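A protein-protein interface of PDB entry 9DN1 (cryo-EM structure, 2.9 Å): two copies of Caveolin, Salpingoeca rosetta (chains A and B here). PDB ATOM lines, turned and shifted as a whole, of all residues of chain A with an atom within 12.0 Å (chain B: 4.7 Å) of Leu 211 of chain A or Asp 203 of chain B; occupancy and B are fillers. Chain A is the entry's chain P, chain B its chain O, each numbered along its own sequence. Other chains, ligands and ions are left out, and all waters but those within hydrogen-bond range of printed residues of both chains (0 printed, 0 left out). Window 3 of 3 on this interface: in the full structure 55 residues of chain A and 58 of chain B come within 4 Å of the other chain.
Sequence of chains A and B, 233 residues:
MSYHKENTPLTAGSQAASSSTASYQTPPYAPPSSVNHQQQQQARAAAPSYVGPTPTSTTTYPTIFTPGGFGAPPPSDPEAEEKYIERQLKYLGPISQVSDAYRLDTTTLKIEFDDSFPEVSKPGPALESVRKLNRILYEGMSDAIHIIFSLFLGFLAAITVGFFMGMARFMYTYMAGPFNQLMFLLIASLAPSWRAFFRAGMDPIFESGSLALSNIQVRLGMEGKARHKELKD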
ATOM      1  N   MET A 202      22.214 -35.218 -34.711  1.00  0.00           N
ATOM      2  CA  MET A 202      21.722 -34.827 -33.394  1.00  0.00           C
ATOM      3  C   MET A 202      20.898 -33.544 -33.376  1.00  0.00           C
ATOM      4  O   MET A 202      20.155 -33.330 -32.414  1.00  0.00           O
ATOM      5  CB  MET A 202      22.894 -34.665 -32.423  1.00  0.00           C
ATOM      6  CG  MET A 202      22.496 -34.815 -30.967  1.00  0.00           C
ATOM      7  SD  MET A 202      22.702 -36.500 -30.365  1.00  0.00           S
ATOM      8  CE  MET A 202      21.756 -36.423 -28.847  1.00  0.00           C
ATOM      9  N   ASP A 203      21.003 -32.684 -34.389  1.00  0.00           N
ATOM     10  CA  ASP A 203      20.337 -31.386 -34.311  1.00  0.00           C
ATOM     11  C   ASP A 203      18.820 -31.470 -34.186  1.00  0.00           C
ATOM     12  O   ASP A 203      18.258 -30.719 -33.371  1.00  0.00           O
ATOM     13  CB  ASP A 203      20.719 -30.530 -35.522  1.00  0.00           C
ATOM     14  CG  ASP A 203      21.967 -29.703 -35.283  1.00  0.00           C
ATOM     15  OD1 ASP A 203      22.567 -29.825 -34.195  1.00  0.00           O
ATOM     16  OD2 ASP A 203      22.343 -28.921 -36.181  1.00  0.00           O
ATOM     17  N   PRO A 204      18.106 -32.314 -34.936  1.00  0.00           N
ATOM     18  CA  PRO A 204      16.636 -32.304 -34.842  1.00  0.00           C
ATOM     19  C   PRO A 204      16.115 -32.419 -33.421  1.00  0.00           C
ATOM     20  O   PRO A 204      15.063 -31.848 -33.096  1.00  0.00           O
ATOM     21  CB  PRO A 204      16.234 -33.518 -35.686  1.00  0.00           C
ATOM     22  CG  PRO A 204      17.325 -33.659 -36.678  1.00  0.00           C
ATOM     23  CD  PRO A 204      18.585 -33.237 -35.979  1.00  0.00           C
ATOM     24  N   ILE A 205      16.833 -33.140 -32.558  1.00  0.00           N
ATOM     25  CA  ILE A 205      16.370 -33.362 -31.193  1.00  0.00           C
ATOM     26  C   ILE A 205      16.280 -32.052 -30.427  1.00  0.00           C
ATOM     27  O   ILE A 205      15.478 -31.926 -29.494  1.00  0.00           O
ATOM     28  CB  ILE A 205      17.299 -34.372 -30.494  1.00  0.00           C
ATOM     29  CG1 ILE A 205      17.057 -35.769 -31.063  1.00  0.00           C
ATOM     30  CG2 ILE A 205      17.071 -34.366 -28.993  1.00  0.00           C
ATOM     31  CD1 ILE A 205      18.204 -36.719 -30.860  1.00  0.00           C
ATOM     32  N   PHE A 206      17.091 -31.061 -30.794  1.00  0.00           N
ATOM     33  CA  PHE A 206      17.051 -29.760 -30.141  1.00  0.00           C
ATOM     34  C   PHE A 206      16.256 -28.727 -30.921  1.00  0.00           C
ATOM     35  O   PHE A 206      15.869 -27.705 -30.345  1.00  0.00           O
ATOM     36  CB  PHE A 206      18.473 -29.242 -29.907  1.00  0.00           C
ATOM     37  CG  PHE A 206      19.251 -30.064 -28.922  1.00  0.00           C
ATOM     38  CD1 PHE A 206      19.022 -29.936 -27.565  1.00  0.00           C
ATOM     39  CD2 PHE A 206      20.201 -30.971 -29.353  1.00  0.00           C
ATOM     40  CE1 PHE A 206      19.729 -30.693 -26.655  1.00  0.00           C
ATOM     41  CE2 PHE A 206      20.911 -31.731 -28.447  1.00  0.00           C
ATOM     42  CZ  PHE A 206      20.675 -31.591 -27.096  1.00  0.00           C
ATOM     43  N   GLU A 207      16.006 -28.960 -32.210  1.00  0.00           N
ATOM     44  CA  GLU A 207      15.037 -28.140 -32.925  1.00  0.00           C
ATOM     45  C   GLU A 207      13.626 -28.413 -32.427  1.00  0.00           C
ATOM     46  O   GLU A 207      12.818 -27.488 -32.290  1.00  0.00           O
ATOM     47  CB  GLU A 207      15.130 -28.400 -34.425  1.00  0.00           C
ATOM     48  CG  GLU A 207      16.343 -27.788 -35.087  1.00  0.00           C
ATOM     49  CD  GLU A 207      16.270 -27.858 -36.598  1.00  0.00           C
ATOM     50  OE1 GLU A 207      15.254 -27.408 -37.165  1.00  0.00           O
ATOM     51  OE2 GLU A 207      17.226 -28.368 -37.217  1.00  0.00           O
ATOM     52  N   SER A 208      13.309 -29.681 -32.155  1.00  0.00           N
ATOM     53  CA  SER A 208      12.006 -30.002 -31.581  1.00  0.00           C
ATOM     54  C   SER A 208      11.854 -29.400 -30.190  1.00  0.00           C
ATOM     55  O   SER A 208      10.801 -28.842 -29.862  1.00  0.00           O
ATOM     56  CB  SER A 208      11.812 -31.515 -31.527  1.00  0.00           C
ATOM     57  OG  SER A 208      11.772 -32.069 -32.829  1.00  0.00           O
ATOM     58  N   GLY A 209      12.895 -29.494 -29.362  1.00  0.00           N
ATOM     59  CA  GLY A 209      12.821 -28.962 -28.014  1.00  0.00           C
ATOM     60  C   GLY A 209      12.735 -27.454 -27.955  1.00  0.00           C
ATOM     61  O   GLY A 209      12.420 -26.902 -26.897  1.00  0.00           O
ATOM     62  N   SER A 210      13.009 -26.775 -29.070  1.00  0.00           N
ATOM     63  CA  SER A 210      12.964 -25.320 -29.096  1.00  0.00           C
ATOM     64  C   SER A 210      11.544 -24.778 -29.017  1.00  0.00           C
ATOM     65  O   SER A 210      11.363 -23.615 -28.649  1.00  0.00           O
ATOM     66  CB  SER A 210      13.636 -24.805 -30.366  1.00  0.00           C
ATOM     67  OG  SER A 210      13.704 -23.393 -30.365  1.00  0.00           O
ATOM     68  N   LEU A 211      10.538 -25.587 -29.351  1.00  0.00           N
ATOM     69  CA  LEU A 211       9.163 -25.108 -29.389  1.00  0.00           C
ATOM     70  C   LEU A 211       8.595 -24.820 -28.009  1.00  0.00           C
ATOM     71  O   LEU A 211       7.510 -24.238 -27.918  1.00  0.00           O
ATOM     72  CB  LEU A 211       8.272 -26.129 -30.095  1.00  0.00           C
ATOM     73  CG  LEU A 211       8.629 -26.486 -31.538  1.00  0.00           C
ATOM     74  CD1 LEU A 211       7.625 -27.479 -32.087  1.00  0.00           C
ATOM     75  CD2 LEU A 211       8.676 -25.247 -32.410  1.00  0.00           C
ATOM     76  N   ALA A 212       9.287 -25.214 -26.939  1.00  0.00           N
ATOM     77  CA  ALA A 212       8.747 -25.026 -25.599  1.00  0.00           C
ATOM     78  C   ALA A 212       8.772 -23.571 -25.157  1.00  0.00           C
ATOM     79  O   ALA A 212       7.974 -23.191 -24.293  1.00  0.00           O
ATOM     80  CB  ALA A 212       9.520 -25.881 -24.598  1.00  0.00           C
ATOM     81  N   LEU A 213       9.657 -22.751 -25.719  1.00  0.00           N
ATOM     82  CA  LEU A 213       9.773 -21.354 -25.325  1.00  0.00           C
ATOM     83  C   LEU A 213       9.054 -20.407 -26.271  1.00  0.00           C
ATOM     84  O   LEU A 213       9.182 -19.189 -26.120  1.00  0.00           O
ATOM     85  CB  LEU A 213      11.244 -20.957 -25.210  1.00  0.00           C
ATOM     86  CG  LEU A 213      11.987 -21.622 -24.051  1.00  0.00           C
ATOM     87  CD1 LEU A 213      13.463 -21.308 -24.127  1.00  0.00           C
ATOM     88  CD2 LEU A 213      11.416 -21.183 -22.712  1.00  0.00           C
ATOM     89  N   SER A 214       8.314 -20.926 -27.243  1.00  0.00           N
ATOM     90  CA  SER A 214       7.338 -20.107 -27.931  1.00  0.00           C
ATOM     91  C   SER A 214       6.124 -19.905 -27.028  1.00  0.00           C
ATOM     92  O   SER A 214       6.004 -20.509 -25.957  1.00  0.00           O
ATOM     93  CB  SER A 214       6.914 -20.760 -29.244  1.00  0.00           C
ATOM     94  OG  SER A 214       8.023 -20.936 -30.105  1.00  0.00           O
ATOM     95  N   ASN A 215       5.216 -19.038 -27.459  1.00  0.00           N
ATOM     96  CA  ASN A 215       3.931 -18.887 -26.785  1.00  0.00           C
ATOM     97  C   ASN A 215       4.103 -18.454 -25.331  1.00  0.00           C
ATOM     98  O   ASN A 215       3.489 -19.018 -24.425  1.00  0.00           O
ATOM     99  CB  ASN A 215       3.134 -20.187 -26.866  1.00  0.00           C
ATOM    100  CG  ASN A 215       1.646 -19.977 -26.691  1.00  0.00           C
ATOM    101  OD1 ASN A 215       1.139 -18.868 -26.854  1.00  0.00           O
ATOM    102  ND2 ASN A 215       0.936 -21.047 -26.357  1.00  0.00           N
ATOM    103  N   ILE A 216       4.950 -17.454 -25.101  1.00  0.00           N
ATOM    104  CA  ILE A 216       4.986 -16.770 -23.813  1.00  0.00           C
ATOM    105  C   ILE A 216       4.077 -15.552 -23.896  1.00  0.00           C
ATOM    106  O   ILE A 216       4.058 -14.848 -24.912  1.00  0.00           O
ATOM    107  CB  ILE A 216       6.422 -16.371 -23.436  1.00  0.00           C
ATOM    108  CG1 ILE A 216       7.287 -17.616 -23.233  1.00  0.00           C
ATOM    109  CG2 ILE A 216       6.425 -15.529 -22.165  1.00  0.00           C
ATOM    110  CD1 ILE A 216       8.756 -17.316 -23.033  1.00  0.00           C
ATOM    111  N   GLN A 217       3.311 -15.305 -22.836  1.00  0.00           N
ATOM    112  CA  GLN A 217       2.328 -14.227 -22.826  1.00  0.00           C
ATOM    113  C   GLN A 217       2.263 -13.641 -21.425  1.00  0.00           C
ATOM    114  O   GLN A 217       2.130 -14.385 -20.450  1.00  0.00           O
ATOM    115  CB  GLN A 217       0.960 -14.746 -23.272  1.00  0.00           C
ATOM    116  CG  GLN A 217       0.999 -15.455 -24.615  1.00  0.00           C
ATOM    117  CD  GLN A 217      -0.373 -15.691 -25.202  1.00  0.00           C
ATOM    118  OE1 GLN A 217      -1.304 -14.930 -24.953  1.00  0.00           O
ATOM    119  NE2 GLN A 217      -0.505 -16.748 -25.992  1.00  0.00           N
ATOM    120  N   ARG B 199      11.072 -34.818 -36.576  1.00  0.00           N
ATOM    121  CA  ARG B 199      10.268 -33.698 -36.103  1.00  0.00           C
ATOM    122  C   ARG B 199       8.779 -34.001 -36.210  1.00  0.00           C
ATOM    123  O   ARG B 199       8.008 -33.694 -35.295  1.00  0.00           O
ATOM    124  CB  ARG B 199      10.627 -32.431 -36.875  1.00  0.00           C
ATOM    125  CG  ARG B 199      11.927 -31.805 -36.403  1.00  0.00           C
ATOM    126  CD  ARG B 199      12.082 -30.373 -36.876  1.00  0.00           C
ATOM    127  NE  ARG B 199      10.966 -29.528 -36.471  1.00  0.00           N
ATOM    128  CZ  ARG B 199      10.909 -28.219 -36.672  1.00  0.00           C
ATOM    129  NH1 ARG B 199      11.897 -27.568 -37.261  1.00  0.00           N
ATOM    130  NH2 ARG B 199       9.835 -27.547 -36.270  1.00  0.00           N
ATOM    131  N   GLY B 201       7.227 -36.609 -35.774  1.00  0.00           N
ATOM    132  CA  GLY B 201       6.784 -37.482 -34.707  1.00  0.00           C
ATOM    133  C   GLY B 201       6.958 -36.901 -33.319  1.00  0.00           C
ATOM    134  O   GLY B 201       6.213 -37.264 -32.406  1.00  0.00           O
ATOM    135  N   MET B 202       7.925 -35.998 -33.138  1.00  0.00           N
ATOM    136  CA  MET B 202       8.245 -35.528 -31.794  1.00  0.00           C
ATOM    137  C   MET B 202       7.740 -34.126 -31.472  1.00  0.00           C
ATOM    138  O   MET B 202       7.632 -33.791 -30.288  1.00  0.00           O
ATOM    139  CB  MET B 202       9.760 -35.561 -31.573  1.00  0.00           C
ATOM    140  CG  MET B 202      10.161 -35.570 -30.109  1.00  0.00           C
ATOM    141  SD  MET B 202      10.480 -37.228 -29.487  1.00  0.00           S
ATOM    142  CE  MET B 202      10.384 -36.940 -27.723  1.00  0.00           C
ATOM    143  N   ASP B 203       7.430 -33.297 -32.468  1.00  0.00           N
ATOM    144  CA  ASP B 203       7.094 -31.905 -32.175  1.00  0.00           C
ATOM    145  C   ASP B 203       5.866 -31.734 -31.285  1.00  0.00           C
ATOM    146  O   ASP B 203       5.920 -30.893 -30.371  1.00  0.00           O
ATOM    147  CB  ASP B 203       6.910 -31.126 -33.481  1.00  0.00           C
ATOM    148  CG  ASP B 203       8.204 -30.516 -33.984  1.00  0.00           C
ATOM    149  OD1 ASP B 203       9.256 -30.733 -33.348  1.00  0.00           O
ATOM    150  OD2 ASP B 203       8.169 -29.808 -35.012  1.00  0.00           O
ATOM    151  N   PRO B 204       4.758 -32.453 -31.483  1.00  0.00           N
ATOM    152  CA  PRO B 204       3.571 -32.200 -30.648  1.00  0.00           C
ATOM    153  C   PRO B 204       3.857 -32.224 -29.157  1.00  0.00           C
ATOM    154  O   PRO B 204       3.220 -31.486 -28.390  1.00  0.00           O
ATOM    155  CB  PRO B 204       2.621 -33.332 -31.054  1.00  0.00           C
ATOM    156  CG  PRO B 204       3.003 -33.655 -32.447  1.00  0.00           C
ATOM    157  CD  PRO B 204       4.488 -33.446 -32.535  1.00  0.00           C
ATOM    158  N   ILE B 205       4.808 -33.053 -28.724  1.00  0.00           N
ATOM    159  CA  ILE B 205       5.096 -33.192 -27.303  1.00  0.00           C
ATOM    160  C   ILE B 205       5.601 -31.883 -26.716  1.00  0.00           C
ATOM    161  O   ILE B 205       5.423 -31.624 -25.520  1.00  0.00           O
ATOM    162  CB  ILE B 205       6.099 -34.341 -27.089  1.00  0.00           C
ATOM    163  CG1 ILE B 205       5.401 -35.680 -27.329  1.00  0.00           C
ATOM    164  CG2 ILE B 205       6.682 -34.295 -25.689  1.00  0.00           C
ATOM    165  CD1 ILE B 205       6.337 -36.807 -27.658  1.00  0.00           C
ATOM    166  N   PHE B 206       6.235 -31.042 -27.532  1.00  0.00           N
ATOM    167  CA  PHE B 206       6.721 -29.752 -27.066  1.00  0.00           C
ATOM    168  C   PHE B 206       5.789 -28.602 -27.417  1.00  0.00           C
ATOM    169  O   PHE B 206       5.908 -27.528 -26.821  1.00  0.00           O
ATOM    170  CB  PHE B 206       8.114 -29.473 -27.634  1.00  0.00           C
ATOM    171  CG  PHE B 206       9.165 -30.410 -27.119  1.00  0.00           C
ATOM    172  CD1 PHE B 206       9.692 -30.245 -25.851  1.00  0.00           C
ATOM    173  CD2 PHE B 206       9.618 -31.460 -27.894  1.00  0.00           C
ATOM    174  CE1 PHE B 206      10.652 -31.108 -25.368  1.00  0.00           C
ATOM    175  CE2 PHE B 206      10.580 -32.326 -27.417  1.00  0.00           C
ATOM    176  CZ  PHE B 206      11.097 -32.150 -26.152  1.00  0.00           C
ATOM    177  N   GLU B 207       4.874 -28.796 -28.366  1.00  0.00           N
ATOM    178  CA  GLU B 207       3.800 -27.829 -28.551  1.00  0.00           C
ATOM    179  C   GLU B 207       2.831 -27.865 -27.377  1.00  0.00           C
ATOM    180  O   GLU B 207       2.346 -26.819 -26.932  1.00  0.00           O
ATOM    181  CB  GLU B 207       3.060 -28.103 -29.857  1.00  0.00           C
ATOM    182  CG  GLU B 207       3.826 -27.701 -31.097  1.00  0.00           C
ATOM    183  CD  GLU B 207       2.971 -27.760 -32.344  1.00  0.00           C
ATOM    184  OE1 GLU B 207       1.882 -27.149 -32.347  1.00  0.00           O
ATOM    185  OE2 GLU B 207       3.383 -28.421 -33.320  1.00  0.00           O
ATOM    186  N   SER B 210       4.297 -26.136 -24.335  1.00  0.00           N
ATOM    187  CA  SER B 210       4.443 -24.694 -24.462  1.00  0.00           C
ATOM    188  C   SER B 210       3.366 -23.928 -23.707  1.00  0.00           C
ATOM    189  O   SER B 210       3.571 -22.753 -23.390  1.00  0.00           O
ATOM    190  CB  SER B 210       4.412 -24.300 -25.936  1.00  0.00           C
ATOM    191  OG  SER B 210       4.660 -22.917 -26.095  1.00  0.00           O
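The side-chain carboxylate (OD1) of Asp 203 of chain B is in hydrogen-bond range of the side-chain hydroxyl (OG) of Ser 208 of chain A, at 2.9 Å.
The side-chain hydroxyl (OG) of Ser 210 of chain B sits at hydrogen-bond distance from the backbone carbonyl oxygen (O) of Ser 214 of chain A.
NH1 of Arg 199 of chain B lies within salt-bridge range of OE1 of Glu 207 of chain A (3.4 Å).
The side-chain hydroxyl (OG) of Ser 208 of chain A sits at hydrogen-bond distance from the backbone carbonyl oxygen (O) of Pro 204 of chain A.
OD1 of Asn 215 of chain A is in hydrogen-bond range of NE2 of Gln 217 of chain A (2.8 Å).
The guanidinium group (NH2) of Arg 199 of chain B is in salt-bridge range of the side-chain carboxylate (OD2) of Asp 203 of chain B (3.1 Å).
Among the printed residues, merely in contact across the chains: Ser 208 of chain A with Arg 199 of chain B (3.6 Å), Ser 208 of chain A with Phe 206 of chain B (3.5 Å), Leu 211 of chain A with Asp 203 of chain B (3.6 Å), Leu 211 of chain A with Phe 206 of chain B (3.8 Å), Leu 211 of chain A with Glu 207 of chain B (3.9 Å), Leu 211 of chain A with Ser 210 of chain B (3.6 Å), Ala 212 of chain A with Phe 206 of chain B (3.98 Å), Ala 212 of chain A with Ser 210 of chain B (3.8 Å) and Asn 215 of chain A with Ser 210 of chain B (3.2 Å).
Met 202 of chain A touches none of the printed residues of chain B.
Of the printed residues of chain B, Ser 208 of chain A touches Arg 199, Asp 203 and Phe 206.
Leu 211 of chain A touches four residues of chain B.
Of the printed residues of chain B, Ala 212 of chain A touches Phe 206 (3.98 Å) and Ser 210 (3.8 Å).
Of the printed residues of chain B, Ser 214 of chain A touches Ser 210 (2.8 Å).
Arg 199 of chain B touches just these residues of chain A: Glu 207 and Ser 208.
No residue of chain A comes within 4 Å of Gly 201 of chain B.
No residue of chain A comes within 4 Å of Met 202 of chain B.
Of chain A, only Ser 208 and Leu 211 come within 4 Å of Asp 203 of chain B.
Printed residues of chain A within 4 Å of Phe 206 of chain B: Ser 208 (3.5 Å), Leu 211 (3.8 Å) and Ala 212 (3.98 Å).
Glu 207 of chain B touches just one residue of chain A: Leu 211 (3.9 Å).
Ser 210 of chain B touches just these residues of chain A: Leu 211, Ala 212, Ser 214 and Asn 215.
The nearest residue of chain B that does not touch Leu 211 of chain A is Arg 199 of chain B (4.6 Å).
The nearest residue of chain A that does not touch Asp 203 of chain B is Glu 207 of chain A (4.9 Å).
Hydrophobic or aromatic side chains of chain A that line the printed part of chain B: Leu 211.
Of the 9 printed residues of chain B, 5 touch a printed residue of chain A.
Hydrophobic or aromatic side chains of chain B within 4 Å of the printed part of chain A: Phe 206.
Among the printed residues, 12 pairs touch across the chains.
7 positions are printed for both chains.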
